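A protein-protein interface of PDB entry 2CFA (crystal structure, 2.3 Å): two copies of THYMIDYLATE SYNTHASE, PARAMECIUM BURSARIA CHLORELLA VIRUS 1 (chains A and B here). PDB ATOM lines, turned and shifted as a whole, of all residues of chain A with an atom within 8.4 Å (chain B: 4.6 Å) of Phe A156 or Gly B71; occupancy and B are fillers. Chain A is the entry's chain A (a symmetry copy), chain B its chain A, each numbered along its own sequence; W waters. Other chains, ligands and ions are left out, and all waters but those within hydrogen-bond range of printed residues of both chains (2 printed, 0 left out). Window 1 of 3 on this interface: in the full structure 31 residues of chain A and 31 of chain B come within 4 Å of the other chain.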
ATOM      1  N   ARG A  70     -19.592   5.345 -14.247  1.00  0.00           N
ATOM      2  CA  ARG A  70     -18.625   4.910 -15.283  1.00  0.00           C
ATOM      3  C   ARG A  70     -17.531   5.960 -15.559  1.00  0.00           C
ATOM      4  O   ARG A  70     -16.370   5.612 -15.750  1.00  0.00           O
ATOM      5  CB  ARG A  70     -19.321   4.536 -16.597  1.00  0.00           C
ATOM      6  CG  ARG A  70     -20.227   3.297 -16.560  1.00  0.00           C
ATOM      7  CD  ARG A  70     -19.510   2.018 -16.106  1.00  0.00           C
ATOM      8  NE  ARG A  70     -18.172   1.852 -16.682  1.00  0.00           N
ATOM      9  CZ  ARG A  70     -17.207   1.099 -16.151  1.00  0.00           C
ATOM     10  NH1 ARG A  70     -16.025   1.007 -16.753  1.00  0.00           N
ATOM     11  NH2 ARG A  70     -17.417   0.430 -15.021  1.00  0.00           N
ATOM     12  N   ALA A  74     -13.561   5.219 -14.993  1.00  0.00           N
ATOM     13  CA  ALA A  74     -12.526   5.373 -16.035  1.00  0.00           C
ATOM     14  C   ALA A  74     -11.293   6.148 -15.542  1.00  0.00           C
ATOM     15  O   ALA A  74     -10.180   5.830 -15.926  1.00  0.00           O
ATOM     16  CB  ALA A  74     -13.097   6.025 -17.288  1.00  0.00           C
ATOM     17  N   LEU A  77      -9.434   3.822 -13.055  1.00  0.00           N
ATOM     18  CA  LEU A  77      -8.691   2.838 -13.873  1.00  0.00           C
ATOM     19  C   LEU A  77      -7.275   3.275 -14.263  1.00  0.00           C
ATOM     20  O   LEU A  77      -6.429   2.427 -14.574  1.00  0.00           O
ATOM     21  CB  LEU A  77      -9.482   2.503 -15.143  1.00  0.00           C
ATOM     22  CG  LEU A  77     -10.437   1.298 -15.200  1.00  0.00           C
ATOM     23  CD1 LEU A  77     -10.810   0.695 -13.830  1.00  0.00           C
ATOM     24  CD2 LEU A  77     -11.686   1.620 -16.028  1.00  0.00           C
ATOM     25  N   GLU A  86     -14.349  -5.761 -12.876  1.00  0.00           N
ATOM     26  CA  GLU A  86     -15.631  -5.190 -13.242  1.00  0.00           C
ATOM     27  C   GLU A  86     -16.639  -6.306 -13.465  1.00  0.00           C
ATOM     28  O   GLU A  86     -16.274  -7.442 -13.746  1.00  0.00           O
ATOM     29  CB  GLU A  86     -15.482  -4.292 -14.473  1.00  0.00           C
ATOM     30  CG  GLU A  86     -14.594  -3.077 -14.192  1.00  0.00           C
ATOM     31  CD  GLU A  86     -14.208  -2.320 -15.439  1.00  0.00           C
ATOM     32  OE1 GLU A  86     -13.121  -2.603 -15.992  1.00  0.00           O
ATOM     33  OE2 GLU A  86     -14.991  -1.448 -15.866  1.00  0.00           O
ATOM     34  N   SER A 137     -32.695   7.329 -21.874  1.00  0.00           N
ATOM     35  CA  SER A 137     -31.601   6.440 -22.273  1.00  0.00           C
ATOM     36  C   SER A 137     -31.813   5.026 -21.740  1.00  0.00           C
ATOM     37  O   SER A 137     -31.516   4.048 -22.428  1.00  0.00           O
ATOM     38  CB  SER A 137     -30.255   6.983 -21.792  1.00  0.00           C
ATOM     39  OG  SER A 137     -29.975   8.246 -22.367  1.00  0.00           O
ATOM     40  N   TYR A 141     -32.524   1.511 -23.758  1.00  0.00           N
ATOM     41  CA  TYR A 141     -31.668   0.405 -23.333  1.00  0.00           C
ATOM     42  C   TYR A 141     -32.497  -0.853 -23.057  1.00  0.00           C
ATOM     43  O   TYR A 141     -32.192  -1.928 -23.579  1.00  0.00           O
ATOM     44  CB  TYR A 141     -30.848   0.803 -22.099  1.00  0.00           C
ATOM     45  CG  TYR A 141     -29.990  -0.307 -21.525  1.00  0.00           C
ATOM     46  CD1 TYR A 141     -30.352  -0.947 -20.341  1.00  0.00           C
ATOM     47  CD2 TYR A 141     -28.820  -0.717 -22.167  1.00  0.00           C
ATOM     48  CE1 TYR A 141     -29.569  -1.968 -19.807  1.00  0.00           C
ATOM     49  CE2 TYR A 141     -28.028  -1.735 -21.641  1.00  0.00           C
ATOM     50  CZ  TYR A 141     -28.409  -2.355 -20.463  1.00  0.00           C
ATOM     51  OH  TYR A 141     -27.632  -3.361 -19.940  1.00  0.00           O
ATOM     52  N   ALA A 150     -27.910  -7.405 -28.250  1.00  0.00           N
ATOM     53  CA  ALA A 150     -26.900  -7.864 -27.292  1.00  0.00           C
ATOM     54  C   ALA A 150     -26.581  -6.830 -26.210  1.00  0.00           C
ATOM     55  O   ALA A 150     -26.697  -5.622 -26.432  1.00  0.00           O
ATOM     56  CB  ALA A 150     -25.630  -8.285 -28.022  1.00  0.00           C
ATOM     57  N   LYS A 151     -26.191  -7.328 -25.039  1.00  0.00           N
ATOM     58  CA  LYS A 151     -25.822  -6.497 -23.896  1.00  0.00           C
ATOM     59  C   LYS A 151     -24.691  -5.512 -24.202  1.00  0.00           C
ATOM     60  O   LYS A 151     -24.717  -4.374 -23.733  1.00  0.00           O
ATOM     61  CB  LYS A 151     -25.418  -7.384 -22.713  1.00  0.00           C
ATOM     62  CG  LYS A 151     -26.513  -7.640 -21.681  1.00  0.00           C
ATOM     63  CD  LYS A 151     -26.772  -6.397 -20.831  1.00  0.00           C
ATOM     64  CE  LYS A 151     -26.969  -6.742 -19.360  1.00  0.00           C
ATOM     65  NZ  LYS A 151     -25.661  -6.966 -18.667  1.00  0.00           N
ATOM     66  N   GLU A 152     -23.713  -5.953 -24.992  1.00  0.00           N
ATOM     67  CA  GLU A 152     -22.506  -5.168 -25.267  1.00  0.00           C
ATOM     68  C   GLU A 152     -22.745  -4.059 -26.289  1.00  0.00           C
ATOM     69  O   GLU A 152     -22.015  -3.066 -26.309  1.00  0.00           O
ATOM     70  CB  GLU A 152     -21.345  -6.064 -25.727  1.00  0.00           C
ATOM     71  CG  GLU A 152     -21.064  -7.267 -24.828  1.00  0.00           C
ATOM     72  CD  GLU A 152     -21.899  -8.480 -25.202  1.00  0.00           C
ATOM     73  OE1 GLU A 152     -22.848  -8.806 -24.454  1.00  0.00           O
ATOM     74  OE2 GLU A 152     -21.616  -9.097 -26.253  1.00  0.00           O
ATOM     75  N   CYS A 153     -23.759  -4.239 -27.134  1.00  0.00           N
ATOM     76  CA  CYS A 153     -24.173  -3.215 -28.097  1.00  0.00           C
ATOM     77  C   CYS A 153     -25.050  -2.150 -27.438  1.00  0.00           C
ATOM     78  O   CYS A 153     -24.896  -0.953 -27.698  1.00  0.00           O
ATOM     79  CB  CYS A 153     -24.920  -3.850 -29.273  1.00  0.00           C
ATOM     80  SG  CYS A 153     -23.852  -4.580 -30.534  1.00  0.00           S
ATOM     81  N   ALA A 154     -25.970  -2.603 -26.590  1.00  0.00           N
ATOM     82  CA  ALA A 154     -26.890  -1.729 -25.876  1.00  0.00           C
ATOM     83  C   ALA A 154     -26.169  -0.841 -24.857  1.00  0.00           C
ATOM     84  O   ALA A 154     -26.538   0.322 -24.675  1.00  0.00           O
ATOM     85  CB  ALA A 154     -27.974  -2.554 -25.204  1.00  0.00           C
ATOM     86  N   ARG A 155     -25.140  -1.398 -24.212  1.00  0.00           N
ATOM     87  CA  ARG A 155     -24.274  -0.677 -23.265  1.00  0.00           C
ATOM     88  C   ARG A 155     -23.747   0.671 -23.764  1.00  0.00           C
ATOM     89  O   ARG A 155     -23.514   1.580 -22.969  1.00  0.00           O
ATOM     90  CB  ARG A 155     -23.089  -1.557 -22.851  1.00  0.00           C
ATOM     91  CG  ARG A 155     -23.061  -1.917 -21.372  1.00  0.00           C
ATOM     92  CD  ARG A 155     -21.880  -2.832 -21.006  1.00  0.00           C
ATOM     93  NE  ARG A 155     -20.616  -2.419 -21.622  1.00  0.00           N
ATOM     94  CZ  ARG A 155     -19.765  -1.527 -21.115  1.00  0.00           C
ATOM     95  NH1 ARG A 155     -18.655  -1.241 -21.779  1.00  0.00           N
ATOM     96  NH2 ARG A 155     -20.012  -0.917 -19.959  1.00  0.00           N
ATOM     97  N   PHE A 156     -23.568   0.794 -25.075  1.00  0.00           N
ATOM     98  CA  PHE A 156     -22.994   1.999 -25.671  1.00  0.00           C
ATOM     99  C   PHE A 156     -23.882   3.242 -25.647  1.00  0.00           C
ATOM    100  O   PHE A 156     -23.399   4.345 -25.908  1.00  0.00           O
ATOM    101  CB  PHE A 156     -22.520   1.719 -27.101  1.00  0.00           C
ATOM    102  CG  PHE A 156     -21.161   1.093 -27.169  1.00  0.00           C
ATOM    103  CD1 PHE A 156     -20.022   1.841 -26.881  1.00  0.00           C
ATOM    104  CD2 PHE A 156     -21.017  -0.246 -27.511  1.00  0.00           C
ATOM    105  CE1 PHE A 156     -18.755   1.265 -26.937  1.00  0.00           C
ATOM    106  CE2 PHE A 156     -19.751  -0.834 -27.569  1.00  0.00           C
ATOM    107  CZ  PHE A 156     -18.619  -0.074 -27.282  1.00  0.00           C
ATOM    108  N   ILE A 157     -25.166   3.070 -25.341  1.00  0.00           N
ATOM    109  CA  ILE A 157     -26.084   4.210 -25.267  1.00  0.00           C
ATOM    110  C   ILE A 157     -26.145   4.795 -23.844  1.00  0.00           C
ATOM    111  O   ILE A 157     -26.653   5.898 -23.626  1.00  0.00           O
ATOM    112  CB  ILE A 157     -27.492   3.866 -25.858  1.00  0.00           C
ATOM    113  CG1 ILE A 157     -28.115   5.101 -26.500  1.00  0.00           C
ATOM    114  CG2 ILE A 157     -28.421   3.238 -24.814  1.00  0.00           C
ATOM    115  CD1 ILE A 157     -28.924   4.795 -27.744  1.00  0.00           C
ATOM    116  N   LEU A 158     -25.592   4.047 -22.894  1.00  0.00           N
ATOM    117  CA  LEU A 158     -25.517   4.454 -21.495  1.00  0.00           C
ATOM    118  C   LEU A 158     -24.567   5.642 -21.299  1.00  0.00           C
ATOM    119  O   LEU A 158     -23.469   5.651 -21.854  1.00  0.00           O
ATOM    120  CB  LEU A 158     -25.072   3.263 -20.640  1.00  0.00           C
ATOM    121  CG  LEU A 158     -26.089   2.313 -19.983  1.00  0.00           C
ATOM    122  CD1 LEU A 158     -27.419   2.199 -20.723  1.00  0.00           C
ATOM    123  CD2 LEU A 158     -25.451   0.934 -19.765  1.00  0.00           C
ATOM    124  N   PRO A 159     -25.002   6.659 -20.530  1.00  0.00           N
ATOM    125  CA  PRO A 159     -24.180   7.841 -20.256  1.00  0.00           C
ATOM    126  C   PRO A 159     -23.058   7.562 -19.248  1.00  0.00           C
ATOM    127  O   PRO A 159     -23.141   6.582 -18.515  1.00  0.00           O
ATOM    128  CB  PRO A 159     -25.193   8.834 -19.671  1.00  0.00           C
ATOM    129  CG  PRO A 159     -26.228   7.991 -19.052  1.00  0.00           C
ATOM    130  CD  PRO A 159     -26.331   6.754 -19.895  1.00  0.00           C
ATOM    131  N   LEU A 160     -22.031   8.417 -19.205  1.00  0.00           N
ATOM    132  CA  LEU A 160     -20.926   8.259 -18.245  1.00  0.00           C
ATOM    133  C   LEU A 160     -21.356   8.360 -16.769  1.00  0.00           C
ATOM    134  O   LEU A 160     -20.612   7.975 -15.868  1.00  0.00           O
ATOM    135  CB  LEU A 160     -19.796   9.266 -18.516  1.00  0.00           C
ATOM    136  CG  LEU A 160     -18.700   9.057 -19.579  1.00  0.00           C
ATOM    137  CD1 LEU A 160     -18.588   7.625 -20.018  1.00  0.00           C
ATOM    138  CD2 LEU A 160     -18.886   9.923 -20.790  1.00  0.00           C
ATOM    139  N   SER B  69     -14.283   4.610 -29.177  1.00  0.00           N
ATOM    140  CA  SER B  69     -15.331   5.142 -28.298  1.00  0.00           C
ATOM    141  C   SER B  69     -14.853   5.155 -26.845  1.00  0.00           C
ATOM    142  O   SER B  69     -13.911   4.445 -26.510  1.00  0.00           O
ATOM    143  CB  SER B  69     -16.583   4.271 -28.419  1.00  0.00           C
ATOM    144  OG  SER B  69     -16.296   2.931 -28.048  1.00  0.00           O
ATOM    145  N   ARG B  70     -15.496   5.944 -25.980  1.00  0.00           N
ATOM    146  CA  ARG B  70     -15.200   5.886 -24.529  1.00  0.00           C
ATOM    147  C   ARG B  70     -15.353   4.468 -23.943  1.00  0.00           C
ATOM    148  O   ARG B  70     -14.557   4.052 -23.108  1.00  0.00           O
ATOM    149  CB  ARG B  70     -16.063   6.867 -23.729  1.00  0.00           C
ATOM    150  CG  ARG B  70     -15.807   8.361 -23.979  1.00  0.00           C
ATOM    151  CD  ARG B  70     -14.358   8.794 -23.720  1.00  0.00           C
ATOM    152  NE  ARG B  70     -13.771   8.208 -22.510  1.00  0.00           N
ATOM    153  CZ  ARG B  70     -12.461   8.072 -22.293  1.00  0.00           C
ATOM    154  NH1 ARG B  70     -12.026   7.533 -21.158  1.00  0.00           N
ATOM    155  NH2 ARG B  70     -11.580   8.480 -23.201  1.00  0.00           N
ATOM    156  N   GLY B  71     -16.370   3.740 -24.399  1.00  0.00           N
ATOM    157  CA  GLY B  71     -16.632   2.350 -23.981  1.00  0.00           C
ATOM    158  C   GLY B  71     -15.508   1.352 -24.247  1.00  0.00           C
ATOM    159  O   GLY B  71     -15.172   0.534 -23.386  1.00  0.00           O
ATOM    160  N   ILE B  72     -14.929   1.423 -25.442  1.00  0.00           N
ATOM    161  CA  ILE B  72     -13.819   0.564 -25.822  1.00  0.00           C
ATOM    162  C   ILE B  72     -12.532   1.031 -25.144  1.00  0.00           C
ATOM    163  O   ILE B  72     -11.736   0.209 -24.688  1.00  0.00           O
ATOM    164  CB  ILE B  72     -13.652   0.505 -27.365  1.00  0.00           C
ATOM    165  CG1 ILE B  72     -14.902  -0.112 -28.031  1.00  0.00           C
ATOM    166  CG2 ILE B  72     -12.354  -0.230 -27.768  1.00  0.00           C
ATOM    167  CD1 ILE B  72     -15.251  -1.529 -27.566  1.00  0.00           C
ATOM    168  N   ALA B  73     -12.334   2.348 -25.076  1.00  0.00           N
ATOM    169  CA  ALA B  73     -11.196   2.906 -24.363  1.00  0.00           C
ATOM    170  C   ALA B  73     -11.146   2.424 -22.900  1.00  0.00           C
ATOM    171  O   ALA B  73     -10.098   1.997 -22.432  1.00  0.00           O
ATOM    172  CB  ALA B  73     -11.193   4.430 -24.452  1.00  0.00           C
ATOM    173  N   ALA B  74     -12.272   2.455 -22.188  1.00  0.00           N
ATOM    174  CA  ALA B  74     -12.305   1.909 -20.816  1.00  0.00           C
ATOM    175  C   ALA B  74     -11.805   0.457 -20.739  1.00  0.00           C
ATOM    176  O   ALA B  74     -11.156   0.087 -19.774  1.00  0.00           O
ATOM    177  CB  ALA B  74     -13.698   2.024 -20.210  1.00  0.00           C
ATOM    178  N   GLN B  75     -12.105  -0.349 -21.759  1.00  0.00           N
ATOM    179  CA  GLN B  75     -11.614  -1.718 -21.838  1.00  0.00           C
ATOM    180  C   GLN B  75     -10.111  -1.750 -22.093  1.00  0.00           C
ATOM    181  O   GLN B  75      -9.390  -2.556 -21.507  1.00  0.00           O
ATOM    182  CB  GLN B  75     -12.308  -2.479 -22.969  1.00  0.00           C
ATOM    183  CG  GLN B  75     -13.773  -2.813 -22.759  1.00  0.00           C
ATOM    184  CD  GLN B  75     -14.365  -3.547 -23.972  1.00  0.00           C
ATOM    185  OE1 GLN B  75     -13.635  -4.154 -24.783  1.00  0.00           O
ATOM    186  NE2 GLN B  75     -15.681  -3.474 -24.112  1.00  0.00           N
ATOM    187  N   PRO B 159     -22.762   9.580 -23.871  1.00  0.00           N
ATOM    188  CA  PRO B 159     -22.869   8.119 -23.910  1.00  0.00           C
ATOM    189  C   PRO B 159     -21.512   7.430 -24.101  1.00  0.00           C
ATOM    190  O   PRO B 159     -20.571   8.075 -24.553  1.00  0.00           O
ATOM    191  CB  PRO B 159     -23.773   7.875 -25.125  1.00  0.00           C
ATOM    192  CG  PRO B 159     -23.533   9.028 -26.007  1.00  0.00           C
ATOM    193  CD  PRO B 159     -23.268  10.201 -25.110  1.00  0.00           C
ATOM    194  N   LEU B 160     -21.417   6.137 -23.775  1.00  0.00           N
ATOM    195  CA  LEU B 160     -20.170   5.376 -23.960  1.00  0.00           C
ATOM    196  C   LEU B 160     -19.714   5.265 -25.428  1.00  0.00           C
ATOM    197  O   LEU B 160     -18.569   4.912 -25.707  1.00  0.00           O
ATOM    198  CB  LEU B 160     -20.273   3.968 -23.352  1.00  0.00           C
ATOM    199  CG  LEU B 160     -20.057   3.664 -21.856  1.00  0.00           C
ATOM    200  CD1 LEU B 160     -19.333   4.770 -21.143  1.00  0.00           C
ATOM    201  CD2 LEU B 160     -21.335   3.370 -21.128  1.00  0.00           C
ATOM    202  N   SER B 161     -20.615   5.570 -26.357  1.00  0.00           N
ATOM    203  CA  SER B 161     -20.312   5.517 -27.785  1.00  0.00           C
ATOM    204  C   SER B 161     -19.584   6.759 -28.293  1.00  0.00           C
ATOM    205  O   SER B 161     -19.101   6.761 -29.423  1.00  0.00           O
ATOM    206  CB  SER B 161     -21.596   5.321 -28.587  1.00  0.00           C
ATOM    207  OG  SER B 161     -22.515   6.351 -28.286  1.00  0.00           O
ATOM    208  N   GLN B 188     -14.785  -8.205 -28.080  1.00  0.00           N
ATOM    209  CA  GLN B 188     -15.886  -7.719 -28.912  1.00  0.00           C
ATOM    210  C   GLN B 188     -15.399  -7.039 -30.190  1.00  0.00           C
ATOM    211  O   GLN B 188     -14.269  -6.570 -30.259  1.00  0.00           O
ATOM    212  CB  GLN B 188     -16.885  -6.872 -28.107  1.00  0.00           C
ATOM    213  CG  GLN B 188     -16.497  -5.440 -27.835  1.00  0.00           C
ATOM    214  CD  GLN B 188     -17.593  -4.693 -27.087  1.00  0.00           C
ATOM    215  OE1 GLN B 188     -17.945  -5.048 -25.956  1.00  0.00           O
ATOM    216  NE2 GLN B 188     -18.143  -3.656 -27.717  1.00  0.00           N
ATOM    217  N   GLU B 190     -15.688  -4.256 -32.094  1.00  0.00           N
ATOM    218  CA  GLU B 190     -15.056  -2.934 -32.145  1.00  0.00           C
ATOM    219  C   GLU B 190     -13.624  -2.983 -31.616  1.00  0.00           C
ATOM    220  O   GLU B 190     -12.737  -2.316 -32.145  1.00  0.00           O
ATOM    221  CB  GLU B 190     -15.872  -1.903 -31.362  1.00  0.00           C
ATOM    222  CG  GLU B 190     -17.234  -1.562 -31.975  1.00  0.00           C
ATOM    223  CD  GLU B 190     -18.297  -2.627 -31.707  1.00  0.00           C
ATOM    224  OE1 GLU B 190     -19.099  -2.909 -32.628  1.00  0.00           O
ATOM    225  OE2 GLU B 190     -18.329  -3.185 -30.582  1.00  0.00           O
HETATM  226  O   HOH W   1     -12.841  -1.280 -18.328  1.00  0.00           O
HETATM  227  O   HOH W   2     -16.619   0.217 -20.933  1.00  0.00           O
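The backbone NH of Leu B160 sits at hydrogen-bond distance from the backbone carbonyl oxygen of Phe A156 (3.4 Å).
The backbone NH (N) of Leu B160 is in hydrogen-bond range of the backbone carbonyl oxygen (O) of Leu A158.
The backbone NH (N) of Ser B161 sits at hydrogen-bond distance from the backbone carbonyl oxygen (O) of Phe A156 (3.1 Å).
The side-chain hydroxyl (OG) of Ser B69 sits at hydrogen-bond distance from the backbone NH (N) of Ile B72, at 3.3 Å.
The backbone NH (N) of Arg A70 is in hydrogen-bond range of the backbone carbonyl oxygen (O) of Leu A160, 3.3 Å away.
The side-chain amide nitrogen (NE2) of Gln B75 is in hydrogen-bond range of the side-chain amide oxygen (OE1) of Gln B188, at 3.3 Å.
O of Leu B160 sits at hydrogen-bond distance from N of Gly B71 (2.8 Å).
The side-chain carboxylate of Glu B190 sits at hydrogen-bond distance from the side-chain amide nitrogen of Gln B188, 2.9 Å away.
The backbone carbonyl oxygen of Leu B160 sits at hydrogen-bond distance from the backbone NH of Arg B70, at 3.3 Å.
Among the printed residues, merely in contact across the chains: Glu A152 with Gln B188 (3.6 Å), Arg A155 with Leu B160 (3.4 Å), Phe A156 with Ser B69 (3.2 Å), Phe A156 with Gly B71 (3.8 Å), Phe A156 with Ile B72 (3.7 Å), Phe A156 with Pro B159 (3.6 Å), Phe A156 with Gln B188 (3.3 Å), Ile A157 with Pro B159 (3.8 Å), Leu A158 with Pro B159 (3.3 Å), Pro A159 with Pro B159 (3.9 Å) and Leu A160 with Leu B160 (3.2 Å).
Of chain B, only Ser B69 (3.2 Å), Gly B71 (3.8 Å), Ile B72 (3.7 Å), Pro B159 (3.6 Å), Leu B160 (3.4 Å), Ser B161 (3.1 Å) and Gln B188 (3.3 Å) come within 4 Å of Phe A156.
Of the printed residues of chain B, Leu A158 touches Pro B159 (3.3 Å) and Leu B160 (2.9 Å).
Of the printed residues of chain B, Pro A159 touches Pro B159.
Of chain A, only Phe A156 (3.8 Å) comes within 4 Å of Gly B71.
Printed residues of chain A within 4 Å of Ser B161: Phe A156 (3.1 Å).
Printed residues of chain A within 4 Å of Gln B188: Glu A152 and Phe A156.
The nearest residue of chain A that does not touch Gly B71 is Arg A155 (4.2 Å).
The nearest printed residue of chain A that does not touch Ser B69 is Arg A155 (7.9 Å).
Of the 12 printed residues of chain B, 7 touch a printed residue of chain A.
Printed residues of chain B that touch a printed residue of chain A: Ser B69, Gly B71, Ile B72, Pro B159, Leu B160, Ser B161 and Gln B188.
Pro B159 touches its own counterpart, Pro A159.
Leu A160 touches its own counterpart, Leu B160.
Water W1 bridges the backbone carbonyl oxygen of Ala B74 (2.6 Å) and the side-chain carboxylate of Glu A86 (2.7 Å).
Water W2 bridges NH1 of Arg A155 (2.6 Å) and O of Gly B71 (2.9 Å).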
